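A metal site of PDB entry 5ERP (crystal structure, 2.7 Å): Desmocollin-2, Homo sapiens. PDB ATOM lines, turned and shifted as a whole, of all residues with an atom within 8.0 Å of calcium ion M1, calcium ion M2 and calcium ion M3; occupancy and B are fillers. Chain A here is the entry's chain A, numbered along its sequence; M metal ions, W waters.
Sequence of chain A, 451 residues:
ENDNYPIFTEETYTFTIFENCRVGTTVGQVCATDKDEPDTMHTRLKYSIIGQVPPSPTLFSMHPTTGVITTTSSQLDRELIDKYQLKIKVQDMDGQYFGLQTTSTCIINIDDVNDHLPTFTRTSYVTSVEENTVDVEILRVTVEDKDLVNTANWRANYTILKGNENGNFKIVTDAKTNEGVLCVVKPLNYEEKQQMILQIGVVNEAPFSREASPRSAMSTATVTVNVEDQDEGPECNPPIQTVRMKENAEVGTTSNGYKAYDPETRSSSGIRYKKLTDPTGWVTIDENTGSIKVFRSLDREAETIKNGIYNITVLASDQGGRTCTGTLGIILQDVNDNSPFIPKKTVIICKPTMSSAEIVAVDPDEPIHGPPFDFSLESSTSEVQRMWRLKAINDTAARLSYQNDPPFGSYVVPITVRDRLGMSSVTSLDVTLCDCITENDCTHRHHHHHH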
ATOM      1  N   GLU A 131     -11.216 -32.090 -16.673  1.00  0.00           N
ATOM      2  CA  GLU A 131     -10.609 -32.512 -17.943  1.00  0.00           C
ATOM      3  C   GLU A 131      -9.128 -32.837 -17.779  1.00  0.00           C
ATOM      4  O   GLU A 131      -8.501 -32.454 -16.792  1.00  0.00           O
ATOM      5  CB  GLU A 131     -10.786 -31.421 -19.006  1.00  0.00           C
ATOM      6  CG  GLU A 131     -10.009 -30.143 -18.726  1.00  0.00           C
ATOM      7  CD  GLU A 131     -10.124 -29.143 -19.854  1.00  0.00           C
ATOM      8  OE1 GLU A 131     -10.108 -29.571 -21.029  1.00  0.00           O
ATOM      9  OE2 GLU A 131     -10.244 -27.942 -19.561  1.00  0.00           O
ATOM     10  N   ASN A 132      -8.584 -33.560 -18.761  1.00  0.00           N
ATOM     11  CA  ASN A 132      -7.182 -33.948 -18.761  1.00  0.00           C
ATOM     12  C   ASN A 132      -6.799 -34.666 -17.473  1.00  0.00           C
ATOM     13  O   ASN A 132      -5.655 -34.636 -17.037  1.00  0.00           O
ATOM     14  CB  ASN A 132      -6.295 -32.719 -18.959  1.00  0.00           C
ATOM     15  CG  ASN A 132      -6.567 -32.020 -20.274  1.00  0.00           C
ATOM     16  OD1 ASN A 132      -6.569 -32.642 -21.332  1.00  0.00           O
ATOM     17  ND2 ASN A 132      -6.843 -30.722 -20.204  1.00  0.00           N
ATOM     18  N   LEU A 188     -10.476 -36.510 -20.643  1.00  0.00           N
ATOM     19  CA  LEU A 188     -11.523 -35.826 -21.381  1.00  0.00           C
ATOM     20  C   LEU A 188     -11.067 -34.415 -21.707  1.00  0.00           C
ATOM     21  O   LEU A 188     -10.146 -33.899 -21.087  1.00  0.00           O
ATOM     22  CB  LEU A 188     -12.818 -35.810 -20.570  1.00  0.00           C
ATOM     23  CG  LEU A 188     -13.304 -37.209 -20.167  1.00  0.00           C
ATOM     24  CD1 LEU A 188     -14.252 -37.149 -18.986  1.00  0.00           C
ATOM     25  CD2 LEU A 188     -13.978 -37.880 -21.361  1.00  0.00           C
ATOM     26  N   ASN A 189     -11.722 -33.808 -22.692  1.00  0.00           N
ATOM     27  CA  ASN A 189     -11.364 -32.471 -23.132  1.00  0.00           C
ATOM     28  C   ASN A 189     -12.591 -31.578 -23.191  1.00  0.00           C
ATOM     29  O   ASN A 189     -13.431 -31.739 -24.070  1.00  0.00           O
ATOM     30  CB  ASN A 189     -10.690 -32.534 -24.508  1.00  0.00           C
ATOM     31  CG  ASN A 189      -9.936 -31.263 -24.840  1.00  0.00           C
ATOM     32  OD1 ASN A 189      -9.285 -30.686 -23.978  1.00  0.00           O
ATOM     33  ND2 ASN A 189     -10.037 -30.807 -26.075  1.00  0.00           N
ATOM     34  N   TYR A 190     -12.694 -30.645 -22.248  1.00  0.00           N
ATOM     35  CA  TYR A 190     -13.863 -29.776 -22.157  1.00  0.00           C
ATOM     36  C   TYR A 190     -14.142 -29.051 -23.481  1.00  0.00           C
ATOM     37  O   TYR A 190     -15.271 -28.645 -23.745  1.00  0.00           O
ATOM     38  CB  TYR A 190     -13.695 -28.762 -21.034  1.00  0.00           C
ATOM     39  CG  TYR A 190     -14.817 -27.749 -20.942  1.00  0.00           C
ATOM     40  CD1 TYR A 190     -15.997 -28.040 -20.276  1.00  0.00           C
ATOM     41  CD2 TYR A 190     -14.694 -26.490 -21.537  1.00  0.00           C
ATOM     42  CE1 TYR A 190     -17.029 -27.125 -20.202  1.00  0.00           C
ATOM     43  CE2 TYR A 190     -15.716 -25.568 -21.470  1.00  0.00           C
ATOM     44  CZ  TYR A 190     -16.883 -25.885 -20.802  1.00  0.00           C
ATOM     45  OH  TYR A 190     -17.908 -24.975 -20.722  1.00  0.00           O
ATOM     46  N   GLU A 191     -13.108 -28.885 -24.303  1.00  0.00           N
ATOM     47  CA  GLU A 191     -13.248 -28.131 -25.539  1.00  0.00           C
ATOM     48  C   GLU A 191     -13.858 -28.956 -26.672  1.00  0.00           C
ATOM     49  O   GLU A 191     -14.398 -28.400 -27.625  1.00  0.00           O
ATOM     50  CB  GLU A 191     -11.885 -27.591 -25.965  1.00  0.00           C
ATOM     51  CG  GLU A 191     -11.480 -26.334 -25.205  1.00  0.00           C
ATOM     52  CD  GLU A 191     -10.928 -26.624 -23.816  1.00  0.00           C
ATOM     53  OE1 GLU A 191     -10.959 -25.705 -22.969  1.00  0.00           O
ATOM     54  OE2 GLU A 191     -10.490 -27.763 -23.561  1.00  0.00           O
ATOM     55  N   GLU A 192     -13.777 -30.278 -26.559  1.00  0.00           N
ATOM     56  CA  GLU A 192     -14.424 -31.168 -27.521  1.00  0.00           C
ATOM     57  C   GLU A 192     -15.846 -31.472 -27.062  1.00  0.00           C
ATOM     58  O   GLU A 192     -16.810 -31.236 -27.794  1.00  0.00           O
ATOM     59  CB  GLU A 192     -13.640 -32.458 -27.688  1.00  0.00           C
ATOM     60  CG  GLU A 192     -14.274 -33.450 -28.663  1.00  0.00           C
ATOM     61  CD  GLU A 192     -13.439 -34.689 -28.874  1.00  0.00           C
ATOM     62  OE1 GLU A 192     -13.830 -35.537 -29.712  1.00  0.00           O
ATOM     63  OE2 GLU A 192     -12.400 -34.826 -28.202  1.00  0.00           O
ATOM     64  N   VAL A 227     -18.083 -32.530 -17.853  1.00  0.00           N
ATOM     65  CA  VAL A 227     -16.651 -32.255 -17.857  1.00  0.00           C
ATOM     66  C   VAL A 227     -16.386 -30.850 -17.341  1.00  0.00           C
ATOM     67  O   VAL A 227     -17.065 -29.909 -17.736  1.00  0.00           O
ATOM     68  CB  VAL A 227     -16.055 -32.412 -19.266  1.00  0.00           C
ATOM     69  CG1 VAL A 227     -14.548 -32.240 -19.222  1.00  0.00           C
ATOM     70  CG2 VAL A 227     -16.419 -33.764 -19.866  1.00  0.00           C
ATOM     71  N   GLU A 228     -15.412 -30.724 -16.442  1.00  0.00           N
ATOM     72  CA  GLU A 228     -15.015 -29.419 -15.911  1.00  0.00           C
ATOM     73  C   GLU A 228     -13.882 -28.817 -16.712  1.00  0.00           C
ATOM     74  O   GLU A 228     -12.934 -29.509 -17.099  1.00  0.00           O
ATOM     75  CB  GLU A 228     -14.601 -29.501 -14.445  1.00  0.00           C
ATOM     76  CG  GLU A 228     -15.731 -29.383 -13.448  1.00  0.00           C
ATOM     77  CD  GLU A 228     -15.223 -29.323 -12.021  1.00  0.00           C
ATOM     78  OE1 GLU A 228     -14.364 -30.158 -11.656  1.00  0.00           O
ATOM     79  OE2 GLU A 228     -15.677 -28.440 -11.262  1.00  0.00           O
ATOM     80  N   ASP A 229     -13.979 -27.512 -16.949  1.00  0.00           N
ATOM     81  CA  ASP A 229     -12.974 -26.772 -17.679  1.00  0.00           C
ATOM     82  C   ASP A 229     -11.766 -26.443 -16.798  1.00  0.00           C
ATOM     83  O   ASP A 229     -11.925 -25.927 -15.682  1.00  0.00           O
ATOM     84  CB  ASP A 229     -13.591 -25.481 -18.246  1.00  0.00           C
ATOM     85  CG  ASP A 229     -12.639 -24.716 -19.147  1.00  0.00           C
ATOM     86  OD1 ASP A 229     -11.574 -25.254 -19.494  1.00  0.00           O
ATOM     87  OD2 ASP A 229     -12.964 -23.564 -19.496  1.00  0.00           O
ATOM     88  N   GLN A 230     -10.573 -26.748 -17.300  1.00  0.00           N
ATOM     89  CA  GLN A 230      -9.332 -26.280 -16.706  1.00  0.00           C
ATOM     90  C   GLN A 230      -8.787 -25.116 -17.509  1.00  0.00           C
ATOM     91  O   GLN A 230      -8.825 -25.143 -18.737  1.00  0.00           O
ATOM     92  CB  GLN A 230      -8.267 -27.385 -16.687  1.00  0.00           C
ATOM     93  CG  GLN A 230      -8.399 -28.450 -15.624  1.00  0.00           C
ATOM     94  CD  GLN A 230      -7.256 -29.452 -15.701  1.00  0.00           C
ATOM     95  OE1 GLN A 230      -6.621 -29.603 -16.751  1.00  0.00           O
ATOM     96  NE2 GLN A 230      -6.977 -30.112 -14.589  1.00  0.00           N
ATOM     97  N   ASP A 231      -8.264 -24.102 -16.825  1.00  0.00           N
ATOM     98  CA  ASP A 231      -7.610 -22.998 -17.511  1.00  0.00           C
ATOM     99  C   ASP A 231      -6.271 -23.511 -18.033  1.00  0.00           C
ATOM    100  O   ASP A 231      -5.293 -23.590 -17.302  1.00  0.00           O
ATOM    101  CB  ASP A 231      -7.416 -21.803 -16.573  1.00  0.00           C
ATOM    102  CG  ASP A 231      -6.798 -20.609 -17.262  1.00  0.00           C
ATOM    103  OD1 ASP A 231      -6.713 -20.608 -18.501  1.00  0.00           O
ATOM    104  OD2 ASP A 231      -6.401 -19.657 -16.550  1.00  0.00           O
ATOM    105  N   GLU A 232      -6.239 -23.852 -19.323  1.00  0.00           N
ATOM    106  CA  GLU A 232      -5.052 -24.455 -19.922  1.00  0.00           C
ATOM    107  C   GLU A 232      -4.155 -23.420 -20.590  1.00  0.00           C
ATOM    108  O   GLU A 232      -4.555 -22.288 -20.828  1.00  0.00           O
ATOM    109  CB  GLU A 232      -5.464 -25.528 -20.944  1.00  0.00           C
ATOM    110  CG  GLU A 232      -6.148 -26.730 -20.316  1.00  0.00           C
ATOM    111  CD  GLU A 232      -6.905 -27.546 -21.336  1.00  0.00           C
ATOM    112  OE1 GLU A 232      -8.010 -27.131 -21.722  1.00  0.00           O
ATOM    113  OE2 GLU A 232      -6.382 -28.609 -21.736  1.00  0.00           O
ATOM    114  N   GLY A 233      -2.933 -23.842 -20.899  1.00  0.00           N
ATOM    115  CA  GLY A 233      -1.941 -22.984 -21.505  1.00  0.00           C
ATOM    116  C   GLY A 233      -2.038 -22.935 -23.016  1.00  0.00           C
ATOM    117  O   GLY A 233      -2.937 -23.553 -23.592  1.00  0.00           O
ATOM    118  N   PRO A 234      -1.110 -22.231 -23.660  1.00  0.00           N
ATOM    119  CA  PRO A 234      -1.133 -21.992 -25.107  1.00  0.00           C
ATOM    120  C   PRO A 234      -1.031 -23.284 -25.905  1.00  0.00           C
ATOM    121  O   PRO A 234      -0.371 -24.213 -25.463  1.00  0.00           O
ATOM    122  CB  PRO A 234       0.087 -21.097 -25.342  1.00  0.00           C
ATOM    123  CG  PRO A 234       1.010 -21.428 -24.234  1.00  0.00           C
ATOM    124  CD  PRO A 234       0.137 -21.734 -23.054  1.00  0.00           C
ATOM    125  N   GLU A 235      -1.696 -23.321 -27.064  1.00  0.00           N
ATOM    126  CA  GLU A 235      -1.682 -24.502 -27.922  1.00  0.00           C
ATOM    127  C   GLU A 235      -1.060 -24.190 -29.269  1.00  0.00           C
ATOM    128  O   GLU A 235      -1.380 -23.163 -29.886  1.00  0.00           O
ATOM    129  CB  GLU A 235      -3.125 -25.016 -28.105  1.00  0.00           C
ATOM    130  CG  GLU A 235      -3.265 -26.253 -28.982  1.00  0.00           C
ATOM    131  CD  GLU A 235      -4.696 -26.756 -29.056  1.00  0.00           C
ATOM    132  OE1 GLU A 235      -5.585 -26.147 -28.421  1.00  0.00           O
ATOM    133  OE2 GLU A 235      -4.943 -27.759 -29.760  1.00  0.00           O
ATOM    134  N   TYR A 261      -2.487 -20.113 -29.705  1.00  0.00           N
ATOM    135  CA  TYR A 261      -3.686 -19.535 -29.124  1.00  0.00           C
ATOM    136  C   TYR A 261      -4.051 -20.188 -27.794  1.00  0.00           C
ATOM    137  O   TYR A 261      -3.564 -21.279 -27.483  1.00  0.00           O
ATOM    138  CB  TYR A 261      -4.851 -19.648 -30.106  1.00  0.00           C
ATOM    139  CG  TYR A 261      -5.188 -21.060 -30.524  1.00  0.00           C
ATOM    140  CD1 TYR A 261      -5.996 -21.867 -29.736  1.00  0.00           C
ATOM    141  CD2 TYR A 261      -4.700 -21.587 -31.718  1.00  0.00           C
ATOM    142  CE1 TYR A 261      -6.310 -23.152 -30.119  1.00  0.00           C
ATOM    143  CE2 TYR A 261      -5.002 -22.877 -32.103  1.00  0.00           C
ATOM    144  CZ  TYR A 261      -5.805 -23.655 -31.302  1.00  0.00           C
ATOM    145  OH  TYR A 261      -6.112 -24.944 -31.679  1.00  0.00           O
ATOM    146  N   ASP A 262      -4.886 -19.513 -27.015  1.00  0.00           N
ATOM    147  CA  ASP A 262      -5.396 -20.072 -25.772  1.00  0.00           C
ATOM    148  C   ASP A 262      -6.592 -20.970 -26.088  1.00  0.00           C
ATOM    149  O   ASP A 262      -7.466 -20.579 -26.863  1.00  0.00           O
ATOM    150  CB  ASP A 262      -5.794 -18.938 -24.806  1.00  0.00           C
ATOM    151  CG  ASP A 262      -6.109 -19.446 -23.411  1.00  0.00           C
ATOM    152  OD1 ASP A 262      -5.440 -20.393 -22.958  1.00  0.00           O
ATOM    153  OD2 ASP A 262      -7.016 -18.885 -22.770  1.00  0.00           O
ATOM    154  N   PRO A 263      -6.651 -22.177 -25.503  1.00  0.00           N
ATOM    155  CA  PRO A 263      -7.783 -23.068 -25.822  1.00  0.00           C
ATOM    156  C   PRO A 263      -9.133 -22.502 -25.404  1.00  0.00           C
ATOM    157  O   PRO A 263     -10.114 -22.697 -26.120  1.00  0.00           O
ATOM    158  CB  PRO A 263      -7.458 -24.330 -25.025  1.00  0.00           C
ATOM    159  CG  PRO A 263      -5.986 -24.313 -24.870  1.00  0.00           C
ATOM    160  CD  PRO A 263      -5.628 -22.873 -24.693  1.00  0.00           C
ATOM    161  N   GLU A 264      -9.193 -21.812 -24.265  1.00  0.00           N
ATOM    162  CA  GLU A 264     -10.433 -21.224 -23.780  1.00  0.00           C
ATOM    163  C   GLU A 264     -10.822 -19.997 -24.607  1.00  0.00           C
ATOM    164  O   GLU A 264     -11.925 -19.920 -25.141  1.00  0.00           O
ATOM    165  CB  GLU A 264     -10.315 -20.841 -22.306  1.00  0.00           C
ATOM    166  CG  GLU A 264     -10.172 -22.021 -21.357  1.00  0.00           C
ATOM    167  CD  GLU A 264      -8.786 -22.631 -21.360  1.00  0.00           C
ATOM    168  OE1 GLU A 264      -7.796 -21.864 -21.435  1.00  0.00           O
ATOM    169  OE2 GLU A 264      -8.674 -23.871 -21.299  1.00  0.00           O
ATOM    170  N   THR A 265      -9.905 -19.036 -24.691  1.00  0.00           N
ATOM    171  CA  THR A 265     -10.171 -17.756 -25.331  1.00  0.00           C
ATOM    172  C   THR A 265     -10.124 -17.805 -26.857  1.00  0.00           C
ATOM    173  O   THR A 265     -10.779 -17.017 -27.528  1.00  0.00           O
ATOM    174  CB  THR A 265      -9.168 -16.684 -24.860  1.00  0.00           C
ATOM    175  OG1 THR A 265      -9.097 -16.689 -23.425  1.00  0.00           O
ATOM    176  CG2 THR A 265      -9.582 -15.292 -25.339  1.00  0.00           C
ATOM    177  N   ARG A 266      -9.338 -18.747 -27.393  1.00  0.00           N
ATOM    178  CA  ARG A 266      -9.068 -18.823 -28.834  1.00  0.00           C
ATOM    179  C   ARG A 266      -8.359 -17.563 -29.337  1.00  0.00           C
ATOM    180  O   ARG A 266      -8.301 -17.307 -30.535  1.00  0.00           O
ATOM    181  CB  ARG A 266     -10.358 -19.054 -29.640  1.00  0.00           C
ATOM    182  CG  ARG A 266     -11.052 -20.376 -29.344  1.00  0.00           C
ATOM    183  CD  ARG A 266     -10.337 -21.569 -29.970  1.00  0.00           C
ATOM    184  NE  ARG A 266     -10.353 -21.527 -31.432  1.00  0.00           N
ATOM    185  CZ  ARG A 266      -9.910 -22.513 -32.208  1.00  0.00           C
ATOM    186  NH1 ARG A 266      -9.411 -23.621 -31.670  1.00  0.00           N
ATOM    187  NH2 ARG A 266      -9.972 -22.387 -33.528  1.00  0.00           N
ATOM    188  N   ASP A 318       2.516 -18.327 -22.251  1.00  0.00           N
ATOM    189  CA  ASP A 318       1.474 -17.422 -21.803  1.00  0.00           C
ATOM    190  C   ASP A 318       1.986 -16.716 -20.561  1.00  0.00           C
ATOM    191  O   ASP A 318       3.075 -17.008 -20.080  1.00  0.00           O
ATOM    192  CB  ASP A 318       0.157 -18.165 -21.526  1.00  0.00           C
ATOM    193  CG  ASP A 318       0.264 -19.203 -20.411  1.00  0.00           C
ATOM    194  OD1 ASP A 318       1.336 -19.337 -19.777  1.00  0.00           O
ATOM    195  OD2 ASP A 318      -0.749 -19.880 -20.153  1.00  0.00           O
ATOM    196  N   ARG A 322       3.439 -21.253 -18.654  1.00  0.00           N
ATOM    197  CA  ARG A 322       3.294 -22.575 -19.244  1.00  0.00           C
ATOM    198  C   ARG A 322       3.497 -22.484 -20.750  1.00  0.00           C
ATOM    199  O   ARG A 322       3.196 -21.463 -21.376  1.00  0.00           O
ATOM    200  CB  ARG A 322       1.942 -23.217 -18.895  1.00  0.00           C
ATOM    201  CG  ARG A 322       0.740 -22.293 -18.863  1.00  0.00           C
ATOM    202  CD  ARG A 322      -0.388 -22.946 -18.101  1.00  0.00           C
ATOM    203  NE  ARG A 322      -1.677 -22.310 -18.382  1.00  0.00           N
ATOM    204  CZ  ARG A 322      -2.159 -21.257 -17.735  1.00  0.00           C
ATOM    205  NH1 ARG A 322      -1.471 -20.692 -16.741  1.00  0.00           N
ATOM    206  NH2 ARG A 322      -3.342 -20.765 -18.064  1.00  0.00           N
HETATM  207 CA    CA M   1      -9.809 -25.919 -20.935  1.00  0.00          CA
HETATM  208 CA    CA M   2      -8.406 -28.982 -22.965  1.00  0.00          CA
HETATM  209 CA    CA M   3      -6.147 -20.258 -20.745  1.00  0.00          CA
HETATM  210  O   HOH W   1      -7.532 -28.121 -25.154  1.00  0.00           O
HETATM  211  O   HOH W   2      -7.896 -18.324 -20.184  1.00  0.00           O
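Merely in contact with calcium ion M3: Arg 322. Five residues have an atom within 4 Å of calcium ion M3: Asp 231, Glu 232, Asp 262, Glu 264 and Arg 322. The nearest printed residue that does not touch calcium ion M3 is Pro 263 (4.8 Å).
Calcium ion M1 is bound by the side-chain carboxylate of Glu 232 (2.3 Å), the side-chain carboxylate of Glu 191 (2.3 Å), the side-chain carboxylate of Glu 264 (2.4 Å), the side-chain carboxylate of Asp 229 (2.4 Å), the side-chain carboxylate of Glu 131 (2.5 Å) and the backbone carbonyl oxygen of Gln 230 (2.5 Å). Calcium ion M1 has six donor atoms within binding distance.
Calcium ion M2 is bound by the side-chain amide oxygen (OD1) of Asn 189 (2.2 Å), the side-chain carboxylate (OE1) of Glu 232 (2.3 Å), the side-chain carboxylate (OE2) of Glu 232 (2.4 Å), the side-chain carboxylate (OE2) of Glu 191 (2.5 Å), water W1 (2.5 Å) and the side-chain carboxylate (OE1) of Glu 131 (2.6 Å).
The nearest printed residue that does not touch calcium ion M1 is Asp 231 (4.8 Å).
The backbone carbonyl oxygen (O) of Leu 188 lies within hydrogen-bond range of the backbone NH (N) of Asn 132 (2.8 Å). O of Glu 228 sits at hydrogen-bond distance from N of Glu 131 (3.1 Å). The guanidinium group (NH2) of Arg 322 lies within salt-bridge range of the side-chain carboxylate (OD2) of Asp 231, at 3.6 Å. The backbone carbonyl oxygen (O) of Glu 232 sits close to the guanidinium group (NH2) of Arg 322, at 3.4 Å. The guanidinium group of Arg 322 lies within salt-bridge range of the side-chain carboxylate of Asp 318, 3.1 Å away. The side-chain carboxylate of Glu 131 sits close to the backbone NH of Tyr 190, 3.1 Å away. OD2 of Asp 262 lies close to OG1 of Thr 265 (3.1 Å). The side-chain amide nitrogen of Asn 132 sits close to the side-chain carboxylate of Glu 232 (2.7 Å).
Merely in contact with calcium ion M2: Asn 132. Within 4 Å of calcium ion M2: Glu 131, Asn 132, Asn 189, Glu 191 and Glu 232. The nearest printed residue that does not touch calcium ion M2 is Tyr 190 (4.7 Å).
Calcium ion M3 is bound by the side-chain carboxylate (OD1) of Asp 262 (2.3 Å), the side-chain carboxylate (OD1) of Asp 231 (2.3 Å), the side-chain carboxylate (OE1) of Glu 264 (2.4 Å), the backbone carbonyl oxygen (O) of Glu 232 (2.6 Å), the side-chain carboxylate (OD2) of Asp 262 (2.6 Å) and water W2 (2.7 Å).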
